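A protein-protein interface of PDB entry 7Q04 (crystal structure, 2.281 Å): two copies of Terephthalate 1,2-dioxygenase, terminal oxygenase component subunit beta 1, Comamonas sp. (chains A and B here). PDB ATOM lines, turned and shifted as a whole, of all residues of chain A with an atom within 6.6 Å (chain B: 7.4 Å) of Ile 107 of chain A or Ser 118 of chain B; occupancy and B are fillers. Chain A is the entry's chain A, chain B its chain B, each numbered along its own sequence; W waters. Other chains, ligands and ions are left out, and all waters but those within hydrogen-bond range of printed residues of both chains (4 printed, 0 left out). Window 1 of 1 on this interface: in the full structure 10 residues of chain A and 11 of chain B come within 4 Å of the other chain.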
ATOM      1  N   ARG A  76     -13.947  -6.367  18.211  1.00  0.00           N
ATOM      2  CA  ARG A  76     -14.440  -7.365  17.234  1.00  0.00           C
ATOM      3  C   ARG A  76     -14.127  -8.775  17.732  1.00  0.00           C
ATOM      4  O   ARG A  76     -12.969  -9.058  18.173  1.00  0.00           O
ATOM      5  CB  ARG A  76     -13.760  -7.228  15.875  1.00  0.00           C
ATOM      6  CG  ARG A  76     -14.638  -6.648  14.785  1.00  0.00           C
ATOM      7  CD  ARG A  76     -13.842  -6.484  13.502  1.00  0.00           C
ATOM      8  NE  ARG A  76     -14.003  -5.200  12.801  1.00  0.00           N
ATOM      9  CZ  ARG A  76     -13.422  -4.033  13.130  1.00  0.00           C
ATOM     10  NH1 ARG A  76     -13.621  -2.968  12.374  1.00  0.00           N
ATOM     11  NH2 ARG A  76     -12.654  -3.925  14.195  1.00  0.00           N
ATOM     12  N   HIS A  77     -15.128  -9.634  17.632  1.00  0.00           N
ATOM     13  CA  HIS A  77     -14.990 -11.073  17.923  1.00  0.00           C
ATOM     14  C   HIS A  77     -16.169 -11.801  17.303  1.00  0.00           C
ATOM     15  O   HIS A  77     -17.165 -11.154  16.928  1.00  0.00           O
ATOM     16  CB  HIS A  77     -14.860 -11.317  19.429  1.00  0.00           C
ATOM     17  CG  HIS A  77     -16.101 -10.986  20.173  1.00  0.00           C
ATOM     18  ND1 HIS A  77     -16.329  -9.730  20.680  1.00  0.00           N
ATOM     19  CD2 HIS A  77     -17.186 -11.733  20.480  1.00  0.00           C
ATOM     20  CE1 HIS A  77     -17.498  -9.728  21.296  1.00  0.00           C
ATOM     21  NE2 HIS A  77     -18.052 -10.941  21.173  1.00  0.00           N
ATOM     22  N   ARG A  78     -16.036 -13.108  17.199  1.00  0.00           N
ATOM     23  CA  ARG A  78     -17.019 -13.989  16.527  1.00  0.00           C
ATOM     24  C   ARG A  78     -17.238 -15.180  17.449  1.00  0.00           C
ATOM     25  O   ARG A  78     -16.405 -15.361  18.368  1.00  0.00           O
ATOM     26  CB  ARG A  78     -16.521 -14.375  15.123  1.00  0.00           C
ATOM     27  CG  ARG A  78     -16.985 -13.461  13.978  1.00  0.00           C
ATOM     28  CD  ARG A  78     -16.295 -13.620  12.600  1.00  0.00           C
ATOM     29  NE  ARG A  78     -16.294 -15.022  12.226  1.00  0.00           N
ATOM     30  CZ  ARG A  78     -15.417 -15.914  12.668  1.00  0.00           C
ATOM     31  NH1 ARG A  78     -15.574 -17.176  12.314  1.00  0.00           N
ATOM     32  NH2 ARG A  78     -14.394 -15.540  13.434  1.00  0.00           N
ATOM     33  N   TYR A  79     -18.343 -15.879  17.248  1.00  0.00           N
ATOM     34  CA  TYR A  79     -18.723 -17.080  18.023  1.00  0.00           C
ATOM     35  C   TYR A  79     -18.586 -18.276  17.095  1.00  0.00           C
ATOM     36  O   TYR A  79     -18.790 -18.128  15.870  1.00  0.00           O
ATOM     37  CB  TYR A  79     -20.164 -17.025  18.554  1.00  0.00           C
ATOM     38  CG  TYR A  79     -20.439 -16.137  19.737  1.00  0.00           C
ATOM     39  CD1 TYR A  79     -19.443 -15.596  20.530  1.00  0.00           C
ATOM     40  CD2 TYR A  79     -21.747 -15.833  20.066  1.00  0.00           C
ATOM     41  CE1 TYR A  79     -19.742 -14.798  21.629  1.00  0.00           C
ATOM     42  CE2 TYR A  79     -22.072 -15.037  21.158  1.00  0.00           C
ATOM     43  CZ  TYR A  79     -21.070 -14.515  21.959  1.00  0.00           C
ATOM     44  OH  TYR A  79     -21.421 -13.733  23.037  1.00  0.00           O
ATOM     45  N   ARG A  80     -18.295 -19.415  17.701  1.00  0.00           N
ATOM     46  CA  ARG A  80     -18.405 -20.732  17.057  1.00  0.00           C
ATOM     47  C   ARG A  80     -19.209 -21.620  18.005  1.00  0.00           C
ATOM     48  O   ARG A  80     -18.661 -22.028  19.039  1.00  0.00           O
ATOM     49  CB  ARG A  80     -17.003 -21.274  16.745  1.00  0.00           C
ATOM     50  CG  ARG A  80     -17.008 -22.653  16.099  1.00  0.00           C
ATOM     51  CD  ARG A  80     -17.769 -22.743  14.790  1.00  0.00           C
ATOM     52  NE  ARG A  80     -17.216 -21.815  13.819  1.00  0.00           N
ATOM     53  CZ  ARG A  80     -17.871 -21.318  12.784  1.00  0.00           C
ATOM     54  NH1 ARG A  80     -19.121 -21.666  12.576  1.00  0.00           N
ATOM     55  NH2 ARG A  80     -17.270 -20.462  11.977  1.00  0.00           N
ATOM     56  N   LEU A 105     -17.474 -21.154  21.437  1.00  0.00           N
ATOM     57  CA  LEU A 105     -16.115 -20.595  21.436  1.00  0.00           C
ATOM     58  C   LEU A 105     -16.245 -19.113  21.097  1.00  0.00           C
ATOM     59  O   LEU A 105     -17.127 -18.770  20.291  1.00  0.00           O
ATOM     60  CB  LEU A 105     -15.234 -21.302  20.409  1.00  0.00           C
ATOM     61  CG  LEU A 105     -15.164 -22.812  20.492  1.00  0.00           C
ATOM     62  CD1 LEU A 105     -14.341 -23.334  19.326  1.00  0.00           C
ATOM     63  CD2 LEU A 105     -14.576 -23.249  21.816  1.00  0.00           C
ATOM     64  N   ARG A 106     -15.407 -18.288  21.695  1.00  0.00           N
ATOM     65  CA  ARG A 106     -15.235 -16.888  21.302  1.00  0.00           C
ATOM     66  C   ARG A 106     -13.849 -16.748  20.665  1.00  0.00           C
ATOM     67  O   ARG A 106     -12.864 -17.058  21.344  1.00  0.00           O
ATOM     68  CB  ARG A 106     -15.349 -15.962  22.511  1.00  0.00           C
ATOM     69  CG  ARG A 106     -15.301 -14.495  22.111  1.00  0.00           C
ATOM     70  CD  ARG A 106     -15.188 -13.534  23.262  1.00  0.00           C
ATOM     71  NE  ARG A 106     -14.019 -13.805  24.068  1.00  0.00           N
ATOM     72  CZ  ARG A 106     -13.853 -13.356  25.302  1.00  0.00           C
ATOM     73  NH1 ARG A 106     -12.785 -13.693  25.989  1.00  0.00           N
ATOM     74  NH2 ARG A 106     -14.784 -12.632  25.896  1.00  0.00           N
ATOM     75  N   ILE A 107     -13.806 -16.255  19.428  1.00  0.00           N
ATOM     76  CA  ILE A 107     -12.556 -15.942  18.685  1.00  0.00           C
ATOM     77  C   ILE A 107     -12.405 -14.418  18.543  1.00  0.00           C
ATOM     78  O   ILE A 107     -13.235 -13.803  17.819  1.00  0.00           O
ATOM     79  CB  ILE A 107     -12.568 -16.656  17.332  1.00  0.00           C
ATOM     80  CG1 ILE A 107     -12.859 -18.144  17.508  1.00  0.00           C
ATOM     81  CG2 ILE A 107     -11.235 -16.415  16.602  1.00  0.00           C
ATOM     82  CD1 ILE A 107     -14.282 -18.527  17.287  1.00  0.00           C
ATOM     83  N   MET A 108     -11.420 -13.819  19.229  1.00  0.00           N
ATOM     84  CA  MET A 108     -11.128 -12.375  19.077  1.00  0.00           C
ATOM     85  C   MET A 108     -10.537 -12.150  17.675  1.00  0.00           C
ATOM     86  O   MET A 108      -9.854 -13.088  17.182  1.00  0.00           O
ATOM     87  CB  MET A 108     -10.103 -11.914  20.113  1.00  0.00           C
ATOM     88  CG  MET A 108     -10.507 -12.178  21.574  1.00  0.00           C
ATOM     89  SD  MET A 108     -12.141 -11.540  22.029  1.00  0.00           S
ATOM     90  CE  MET A 108     -12.016  -9.763  21.722  1.00  0.00           C
ATOM     91  N   HIS A 109     -10.760 -10.971  17.061  1.00  0.00           N
ATOM     92  CA  HIS A 109     -10.053 -10.497  15.829  1.00  0.00           C
ATOM     93  C   HIS A 109      -8.529 -10.670  15.970  1.00  0.00           C
ATOM     94  O   HIS A 109      -7.903 -10.940  14.956  1.00  0.00           O
ATOM     95  CB  HIS A 109     -10.470  -9.056  15.439  1.00  0.00           C
ATOM     96  CG  HIS A 109     -10.006  -7.975  16.365  1.00  0.00           C
ATOM     97  ND1 HIS A 109      -9.519  -6.756  15.904  1.00  0.00           N
ATOM     98  CD2 HIS A 109      -9.938  -7.905  17.711  1.00  0.00           C
ATOM     99  CE1 HIS A 109      -9.188  -5.996  16.935  1.00  0.00           C
ATOM    100  NE2 HIS A 109      -9.446  -6.670  18.039  1.00  0.00           N
ATOM    101  N   THR A 110      -7.978 -10.576  17.183  1.00  0.00           N
ATOM    102  CA  THR A 110      -6.538 -10.764  17.472  1.00  0.00           C
ATOM    103  C   THR A 110      -6.154 -12.254  17.527  1.00  0.00           C
ATOM    104  O   THR A 110      -4.942 -12.537  17.729  1.00  0.00           O
ATOM    105  CB  THR A 110      -6.149 -10.017  18.747  1.00  0.00           C
ATOM    106  OG1 THR A 110      -7.177 -10.184  19.728  1.00  0.00           O
ATOM    107  CG2 THR A 110      -5.926  -8.549  18.486  1.00  0.00           C
ATOM    108  N   GLY A 111      -7.119 -13.183  17.438  1.00  0.00           N
ATOM    109  CA  GLY A 111      -6.854 -14.622  17.181  1.00  0.00           C
ATOM    110  C   GLY A 111      -7.003 -15.547  18.389  1.00  0.00           C
ATOM    111  O   GLY A 111      -6.911 -16.779  18.205  1.00  0.00           O
ATOM    112  N   GLU A 112      -7.196 -15.007  19.595  1.00  0.00           N
ATOM    113  CA  GLU A 112      -7.358 -15.821  20.835  1.00  0.00           C
ATOM    114  C   GLU A 112      -8.681 -16.578  20.736  1.00  0.00           C
ATOM    115  O   GLU A 112      -9.707 -15.912  20.426  1.00  0.00           O
ATOM    116  CB  GLU A 112      -7.324 -14.937  22.089  1.00  0.00           C
ATOM    117  CG  GLU A 112      -6.000 -14.207  22.314  1.00  0.00           C
ATOM    118  CD  GLU A 112      -5.905 -12.818  21.701  1.00  0.00           C
ATOM    119  OE1 GLU A 112      -6.689 -12.496  20.775  1.00  0.00           O
ATOM    120  OE2 GLU A 112      -5.046 -12.042  22.138  1.00  0.00           O
ATOM    121  N   THR A 113      -8.655 -17.899  20.941  1.00  0.00           N
ATOM    122  CA  THR A 113      -9.850 -18.775  20.950  1.00  0.00           C
ATOM    123  C   THR A 113     -10.079 -19.331  22.351  1.00  0.00           C
ATOM    124  O   THR A 113      -9.175 -19.913  22.866  1.00  0.00           O
ATOM    125  CB  THR A 113      -9.778 -19.921  19.939  1.00  0.00           C
ATOM    126  OG1 THR A 113      -9.586 -19.408  18.635  1.00  0.00           O
ATOM    127  CG2 THR A 113     -11.084 -20.667  19.839  1.00  0.00           C
ATOM    128  N   GLU A 114     -11.265 -19.137  22.937  1.00  0.00           N
ATOM    129  CA  GLU A 114     -11.600 -19.532  24.332  1.00  0.00           C
ATOM    130  C   GLU A 114     -12.978 -20.188  24.351  1.00  0.00           C
ATOM    131  O   GLU A 114     -13.852 -19.727  23.594  1.00  0.00           O
ATOM    132  CB  GLU A 114     -11.636 -18.310  25.233  1.00  0.00           C
ATOM    133  CG  GLU A 114     -10.314 -17.990  25.891  1.00  0.00           C
ATOM    134  CD  GLU A 114     -10.374 -16.647  26.607  1.00  0.00           C
ATOM    135  OE1 GLU A 114     -11.190 -16.484  27.584  1.00  0.00           O
ATOM    136  OE2 GLU A 114      -9.664 -15.737  26.131  1.00  0.00           O
ATOM    137  N   THR B  39      -7.363 -21.754   5.207  1.00  0.00           N
ATOM    138  CA  THR B  39      -7.228 -20.279   5.222  1.00  0.00           C
ATOM    139  C   THR B  39      -7.924 -19.747   6.462  1.00  0.00           C
ATOM    140  O   THR B  39      -8.158 -20.558   7.400  1.00  0.00           O
ATOM    141  CB  THR B  39      -7.747 -19.677   3.916  1.00  0.00           C
ATOM    142  OG1 THR B  39      -7.476 -18.268   3.892  1.00  0.00           O
ATOM    143  CG2 THR B  39      -9.231 -19.941   3.752  1.00  0.00           C
ATOM    144  N   VAL B  41     -10.839 -16.428   8.064  1.00  0.00           N
ATOM    145  CA  VAL B  41     -12.016 -15.574   7.740  1.00  0.00           C
ATOM    146  C   VAL B  41     -11.546 -14.242   7.160  1.00  0.00           C
ATOM    147  O   VAL B  41     -12.288 -13.686   6.336  1.00  0.00           O
ATOM    148  CB  VAL B  41     -12.865 -15.320   8.984  1.00  0.00           C
ATOM    149  CG1 VAL B  41     -13.659 -16.560   9.308  1.00  0.00           C
ATOM    150  CG2 VAL B  41     -12.013 -14.818  10.153  1.00  0.00           C
ATOM    151  N   PRO B 101     -19.649 -26.638  10.389  1.00  0.00           N
ATOM    152  CA  PRO B 101     -18.819 -26.151  11.478  1.00  0.00           C
ATOM    153  C   PRO B 101     -17.857 -27.238  11.981  1.00  0.00           C
ATOM    154  O   PRO B 101     -18.213 -28.416  11.986  1.00  0.00           O
ATOM    155  CB  PRO B 101     -19.815 -25.786  12.596  1.00  0.00           C
ATOM    156  CG  PRO B 101     -21.151 -25.660  11.891  1.00  0.00           C
ATOM    157  CD  PRO B 101     -21.077 -26.608  10.713  1.00  0.00           C
ATOM    158  N   PHE B 102     -16.692 -26.801  12.451  1.00  0.00           N
ATOM    159  CA  PHE B 102     -15.663 -27.693  13.032  1.00  0.00           C
ATOM    160  C   PHE B 102     -14.967 -27.008  14.205  1.00  0.00           C
ATOM    161  O   PHE B 102     -14.825 -25.779  14.274  1.00  0.00           O
ATOM    162  CB  PHE B 102     -14.660 -28.167  11.970  1.00  0.00           C
ATOM    163  CG  PHE B 102     -13.674 -27.133  11.462  1.00  0.00           C
ATOM    164  CD1 PHE B 102     -12.563 -26.777  12.227  1.00  0.00           C
ATOM    165  CD2 PHE B 102     -13.802 -26.580  10.186  1.00  0.00           C
ATOM    166  CE1 PHE B 102     -11.643 -25.846  11.763  1.00  0.00           C
ATOM    167  CE2 PHE B 102     -12.883 -25.652   9.723  1.00  0.00           C
ATOM    168  CZ  PHE B 102     -11.814 -25.279  10.507  1.00  0.00           C
ATOM    169  N   MET B 103     -14.514 -27.852  15.117  1.00  0.00           N
ATOM    170  CA  MET B 103     -13.509 -27.508  16.138  1.00  0.00           C
ATOM    171  C   MET B 103     -12.446 -28.605  16.076  1.00  0.00           C
ATOM    172  O   MET B 103     -12.817 -29.783  16.012  1.00  0.00           O
ATOM    173  CB  MET B 103     -14.142 -27.445  17.524  1.00  0.00           C
ATOM    174  CG  MET B 103     -13.108 -27.097  18.590  1.00  0.00           C
ATOM    175  SD  MET B 103     -13.741 -27.197  20.286  1.00  0.00           S
ATOM    176  CE  MET B 103     -14.205 -28.923  20.255  1.00  0.00           C
ATOM    177  N   VAL B 104     -11.167 -28.240  16.117  1.00  0.00           N
ATOM    178  CA  VAL B 104     -10.068 -29.232  16.227  1.00  0.00           C
ATOM    179  C   VAL B 104      -9.308 -28.961  17.524  1.00  0.00           C
ATOM    180  O   VAL B 104      -8.765 -27.861  17.696  1.00  0.00           O
ATOM    181  CB  VAL B 104      -9.170 -29.152  14.986  1.00  0.00           C
ATOM    182  CG1 VAL B 104      -7.956 -30.074  15.087  1.00  0.00           C
ATOM    183  CG2 VAL B 104      -9.962 -29.442  13.720  1.00  0.00           C
ATOM    184  N   VAL B 115      -7.575 -25.840  22.036  1.00  0.00           N
ATOM    185  CA  VAL B 115      -8.372 -25.566  20.819  1.00  0.00           C
ATOM    186  C   VAL B 115      -7.379 -25.041  19.786  1.00  0.00           C
ATOM    187  O   VAL B 115      -6.838 -23.969  20.008  1.00  0.00           O
ATOM    188  CB  VAL B 115      -9.480 -24.555  21.096  1.00  0.00           C
ATOM    189  CG1 VAL B 115     -10.319 -24.371  19.854  1.00  0.00           C
ATOM    190  CG2 VAL B 115     -10.321 -25.012  22.266  1.00  0.00           C
ATOM    191  N   PHE B 116      -7.104 -25.838  18.768  1.00  0.00           N
ATOM    192  CA  PHE B 116      -6.041 -25.587  17.794  1.00  0.00           C
ATOM    193  C   PHE B 116      -6.589 -24.825  16.596  1.00  0.00           C
ATOM    194  O   PHE B 116      -5.865 -23.968  16.049  1.00  0.00           O
ATOM    195  CB  PHE B 116      -5.464 -26.906  17.308  1.00  0.00           C
ATOM    196  CG  PHE B 116      -4.404 -26.730  16.253  1.00  0.00           C
ATOM    197  CD1 PHE B 116      -3.205 -26.106  16.539  1.00  0.00           C
ATOM    198  CD2 PHE B 116      -4.629 -27.191  14.965  1.00  0.00           C
ATOM    199  CE1 PHE B 116      -2.242 -25.977  15.549  1.00  0.00           C
ATOM    200  CE2 PHE B 116      -3.665 -27.071  13.983  1.00  0.00           C
ATOM    201  CZ  PHE B 116      -2.481 -26.452  14.271  1.00  0.00           C
ATOM    202  N   ALA B 117      -7.820 -25.125  16.207  1.00  0.00           N
ATOM    203  CA  ALA B 117      -8.524 -24.372  15.158  1.00  0.00           C
ATOM    204  C   ALA B 117     -10.028 -24.585  15.297  1.00  0.00           C
ATOM    205  O   ALA B 117     -10.453 -25.607  15.882  1.00  0.00           O
ATOM    206  CB  ALA B 117      -8.042 -24.826  13.812  1.00  0.00           C
ATOM    207  N   SER B 118     -10.816 -23.646  14.770  1.00  0.00           N
ATOM    208  CA  SER B 118     -12.280 -23.784  14.643  1.00  0.00           C
ATOM    209  C   SER B 118     -12.693 -23.036  13.377  1.00  0.00           C
ATOM    210  O   SER B 118     -11.931 -22.161  12.959  1.00  0.00           O
ATOM    211  CB  SER B 118     -12.973 -23.251  15.864  1.00  0.00           C
ATOM    212  OG  SER B 118     -12.834 -21.840  15.962  1.00  0.00           O
ATOM    213  N   GLY B 119     -13.839 -23.357  12.794  1.00  0.00           N
ATOM    214  CA  GLY B 119     -14.338 -22.607  11.638  1.00  0.00           C
ATOM    215  C   GLY B 119     -15.405 -23.380  10.925  1.00  0.00           C
ATOM    216  O   GLY B 119     -16.212 -24.024  11.593  1.00  0.00           O
ATOM    217  N   GLU B 120     -15.432 -23.287   9.606  1.00  0.00           N
ATOM    218  CA  GLU B 120     -16.322 -24.145   8.794  1.00  0.00           C
ATOM    219  C   GLU B 120     -15.593 -24.590   7.536  1.00  0.00           C
ATOM    220  O   GLU B 120     -14.707 -23.898   7.015  1.00  0.00           O
ATOM    221  CB  GLU B 120     -17.660 -23.497   8.445  1.00  0.00           C
ATOM    222  CG  GLU B 120     -17.594 -22.015   8.175  1.00  0.00           C
ATOM    223  CD  GLU B 120     -18.910 -21.346   7.818  1.00  0.00           C
ATOM    224  OE1 GLU B 120     -20.013 -21.911   8.112  1.00  0.00           O
ATOM    225  OE2 GLU B 120     -18.791 -20.274   7.212  1.00  0.00           O
ATOM    226  N   ALA B 139     -11.150 -25.147   4.447  1.00  0.00           N
ATOM    227  CA  ALA B 139     -11.202 -25.041   5.911  1.00  0.00           C
ATOM    228  C   ALA B 139     -11.035 -23.560   6.255  1.00  0.00           C
ATOM    229  O   ALA B 139      -9.900 -23.063   6.297  1.00  0.00           O
ATOM    230  CB  ALA B 139     -10.140 -25.912   6.524  1.00  0.00           C
ATOM    231  N   VAL B 140     -12.144 -22.850   6.432  1.00  0.00           N
ATOM    232  CA  VAL B 140     -12.067 -21.403   6.770  1.00  0.00           C
ATOM    233  C   VAL B 140     -11.966 -21.291   8.273  1.00  0.00           C
ATOM    234  O   VAL B 140     -12.965 -21.506   8.935  1.00  0.00           O
ATOM    235  CB  VAL B 140     -13.245 -20.590   6.214  1.00  0.00           C
ATOM    236  CG1 VAL B 140     -13.110 -19.121   6.614  1.00  0.00           C
ATOM    237  CG2 VAL B 140     -13.359 -20.738   4.710  1.00  0.00           C
ATOM    238  N   CYS B 141     -10.768 -21.010   8.782  1.00  0.00           N
ATOM    239  CA  CYS B 141     -10.496 -20.917  10.240  1.00  0.00           C
ATOM    240  C   CYS B 141     -10.984 -19.584  10.794  1.00  0.00           C
ATOM    241  O   CYS B 141     -10.760 -18.558  10.124  1.00  0.00           O
ATOM    242  CB  CYS B 141      -9.016 -21.124  10.485  1.00  0.00           C
ATOM    243  SG  CYS B 141      -8.552 -22.849  10.168  1.00  0.00           S
ATOM    244  N   ASP B 142     -11.559 -19.615  12.002  1.00  0.00           N
ATOM    245  CA  ASP B 142     -12.057 -18.429  12.737  1.00  0.00           C
ATOM    246  C   ASP B 142     -10.892 -17.521  13.162  1.00  0.00           C
ATOM    247  O   ASP B 142     -11.060 -16.257  13.177  1.00  0.00           O
ATOM    248  CB  ASP B 142     -12.871 -18.876  13.947  1.00  0.00           C
ATOM    249  CG  ASP B 142     -14.180 -19.571  13.574  1.00  0.00           C
ATOM    250  OD1 ASP B 142     -14.731 -19.247  12.485  1.00  0.00           O
ATOM    251  OD2 ASP B 142     -14.617 -20.471  14.349  1.00  0.00           O
ATOM    252  N   SER B 143      -9.736 -18.116  13.470  1.00  0.00           N
ATOM    253  CA  SER B 143      -8.539 -17.397  13.959  1.00  0.00           C
ATOM    254  C   SER B 143      -7.524 -17.250  12.830  1.00  0.00           C
ATOM    255  O   SER B 143      -7.297 -18.220  12.069  1.00  0.00           O
ATOM    256  CB  SER B 143      -7.913 -18.135  15.123  1.00  0.00           C
ATOM    257  OG  SER B 143      -6.818 -17.398  15.643  1.00  0.00           O
ATOM    258  N   THR B 144      -6.907 -16.071  12.751  1.00  0.00           N
ATOM    259  CA  THR B 144      -5.698 -15.783  11.934  1.00  0.00           C
ATOM    260  C   THR B 144      -4.461 -16.460  12.549  1.00  0.00           C
ATOM    261  O   THR B 144      -3.430 -16.488  11.843  1.00  0.00           O
ATOM    262  CB  THR B 144      -5.486 -14.269  11.825  1.00  0.00           C
ATOM    263  OG1 THR B 144      -5.446 -13.705  13.130  1.00  0.00           O
ATOM    264  CG2 THR B 144      -6.562 -13.587  11.008  1.00  0.00           C
ATOM    265  N   VAL B 145      -4.552 -17.004  13.776  1.00  0.00           N
ATOM    266  CA  VAL B 145      -3.374 -17.546  14.516  1.00  0.00           C
ATOM    267  C   VAL B 145      -3.403 -19.078  14.523  1.00  0.00           C
ATOM    268  O   VAL B 145      -4.434 -19.682  14.862  1.00  0.00           O
ATOM    269  CB  VAL B 145      -3.301 -16.984  15.944  1.00  0.00           C
ATOM    270  CG1 VAL B 145      -2.085 -17.531  16.693  1.00  0.00           C
ATOM    271  CG2 VAL B 145      -3.297 -15.466  15.974  1.00  0.00           C
ATOM    272  N   LEU B 154      -6.507 -30.054   8.259  1.00  0.00           N
ATOM    273  CA  LEU B 154      -7.797 -29.953   8.980  1.00  0.00           C
ATOM    274  C   LEU B 154      -8.888 -30.701   8.212  1.00  0.00           C
ATOM    275  O   LEU B 154      -8.815 -30.810   6.953  1.00  0.00           O
ATOM    276  CB  LEU B 154      -8.161 -28.481   9.134  1.00  0.00           C
ATOM    277  CG  LEU B 154      -7.134 -27.655   9.894  1.00  0.00           C
ATOM    278  CD1 LEU B 154      -7.592 -26.201   9.984  1.00  0.00           C
ATOM    279  CD2 LEU B 154      -6.869 -28.270  11.266  1.00  0.00           C
ATOM    280  OXT LEU B 154      -9.799 -31.154   8.911  1.00  0.00           O
HETATM  281  O   HOH W   1      -8.032 -14.009  14.572  1.00  0.00           O
HETATM  282  O   HOH W   2     -19.290 -18.842  10.039  1.00  0.00           O
HETATM  283  O   HOH W   3     -21.221 -22.145  10.228  1.00  0.00           O
HETATM  284  O   HOH W   4     -14.748 -19.462   9.812  1.00  0.00           O
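Hydrophobic or aromatic side chains of chain B that line the printed part of chain A: Val 41, Val 115 and Val 145. Printed residues of chain A that touch a printed residue of chain B: Arg 78, Arg 80, Leu 105, Ile 107, Thr 110, Gly 111 and Thr 113. Hydrophobic or aromatic side chains of chain A that line the printed part of chain B: Leu 105 and Ile 107. Among the printed residues, 12 pairs touch across the chains.
The guanidinium group (NH2) of Arg 78 of chain A is in salt-bridge range of the side-chain carboxylate (OD1) of Asp 142 of chain B, at 3.8 Å. O of Gly 111 of chain A sits at hydrogen-bond distance from OG of Ser 143 of chain B (2.6 Å). The guanidinium group (NH2) of Arg 80 of chain A lies within salt-bridge range of the side-chain carboxylate (OD1) of Asp 142 of chain B. The guanidinium group of Arg 80 of chain A lies within hydrogen-bond range of the backbone carbonyl oxygen of Gly 119 of chain B, at 3.3 Å.
Water W3 bridges the side-chain carboxylate (OE1) of Glu 120 of chain B and the guanidinium group (NH1) of Arg 80 of chain A. Water W4 lies within hydrogen-bond range of the side-chain carboxylate of Asp 142 of chain B, the backbone carbonyl oxygen of Val 140 of chain B, the guanidinium group of Arg 80 of chain A and the guanidinium group of Arg 78 of chain A. Water W1 lies within hydrogen-bond range of N of Thr 144 of chain B, O of His 109 of chain A, N of Gly 111 of chain A and O of Met 108 of chain A. Water W2 bridges OE2 of Glu 120 of chain B (3.2 Å) and NH2 of Arg 80 of chain A (3.2 Å).
Among the printed residues, merely in contact across the chains: Ile 107 of chain A with Asp 142 of chain B (3.4 Å), Arg 78 of chain A with Val 41 of chain B (3.6 Å), Leu 105 of chain A with Ser 118 of chain B (3.7 Å), Thr 113 of chain A with Val 115 of chain B (3.8 Å), Thr 110 of chain A with Val 145 of chain B (3.8 Å), Gly 111 of chain A with Val 145 of chain B (3.8 Å), Ile 107 of chain A with Ser 118 of chain B (3.9 Å) and Ile 107 of chain A with Ser 143 of chain B (3.9 Å).
No position is printed for both chains.
The backbone NH (N) of Ile 107 of chain A sits at hydrogen-bond distance from the backbone carbonyl oxygen (O) of Arg 78 of chain A (2.9 Å). The backbone NH (N) of Leu 105 of chain A lies within hydrogen-bond range of the backbone carbonyl oxygen (O) of Arg 80 of chain A (2.8 Å). The backbone carbonyl oxygen (O) of Ser 118 of chain B sits at hydrogen-bond distance from the backbone NH (N) of Asp 142 of chain B (2.7 Å). N of Val 41 of chain B lies within hydrogen-bond range of O of Cys 141 of chain B (3.0 Å). N of Phe 102 of chain B lies within hydrogen-bond range of O of Gly 119 of chain B, 2.9 Å away. The side-chain hydroxyl (OG) of Ser 143 of chain B lies within hydrogen-bond range of the backbone NH (N) of Val 145 of chain B, 3.0 Å away.
Of chain B, only Ser 118 (3.9 Å), Asp 142 (3.4 Å) and Ser 143 (3.9 Å) come within 4 Å of Ile 107 of chain A. His 109 of chain A touches none of the printed residues of chain B. Of the printed residues of chain B, Gly 111 of chain A touches Ser 143 (2.6 Å) and Val 145 (3.8 Å). Printed residues of chain A within 4 Å of Ser 118 of chain B: Leu 105 and Ile 107. Of the printed residues of chain A, Asp 142 of chain B touches Arg 78, Arg 80 and Ile 107. Printed residues of chain A within 4 Å of Ser 143 of chain B: Ile 107 and Gly 111. The nearest residue of chain B that does not touch Ile 107 of chain A is Thr 144 of chain B (5.8 Å). The nearest residue of chain A that does not touch Ser 118 of chain B is Arg 80 of chain A (4.1 Å). The nearest printed residue of chain B that does not touch Arg 80 of chain A is Ser 118 of chain B (4.1 Å).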
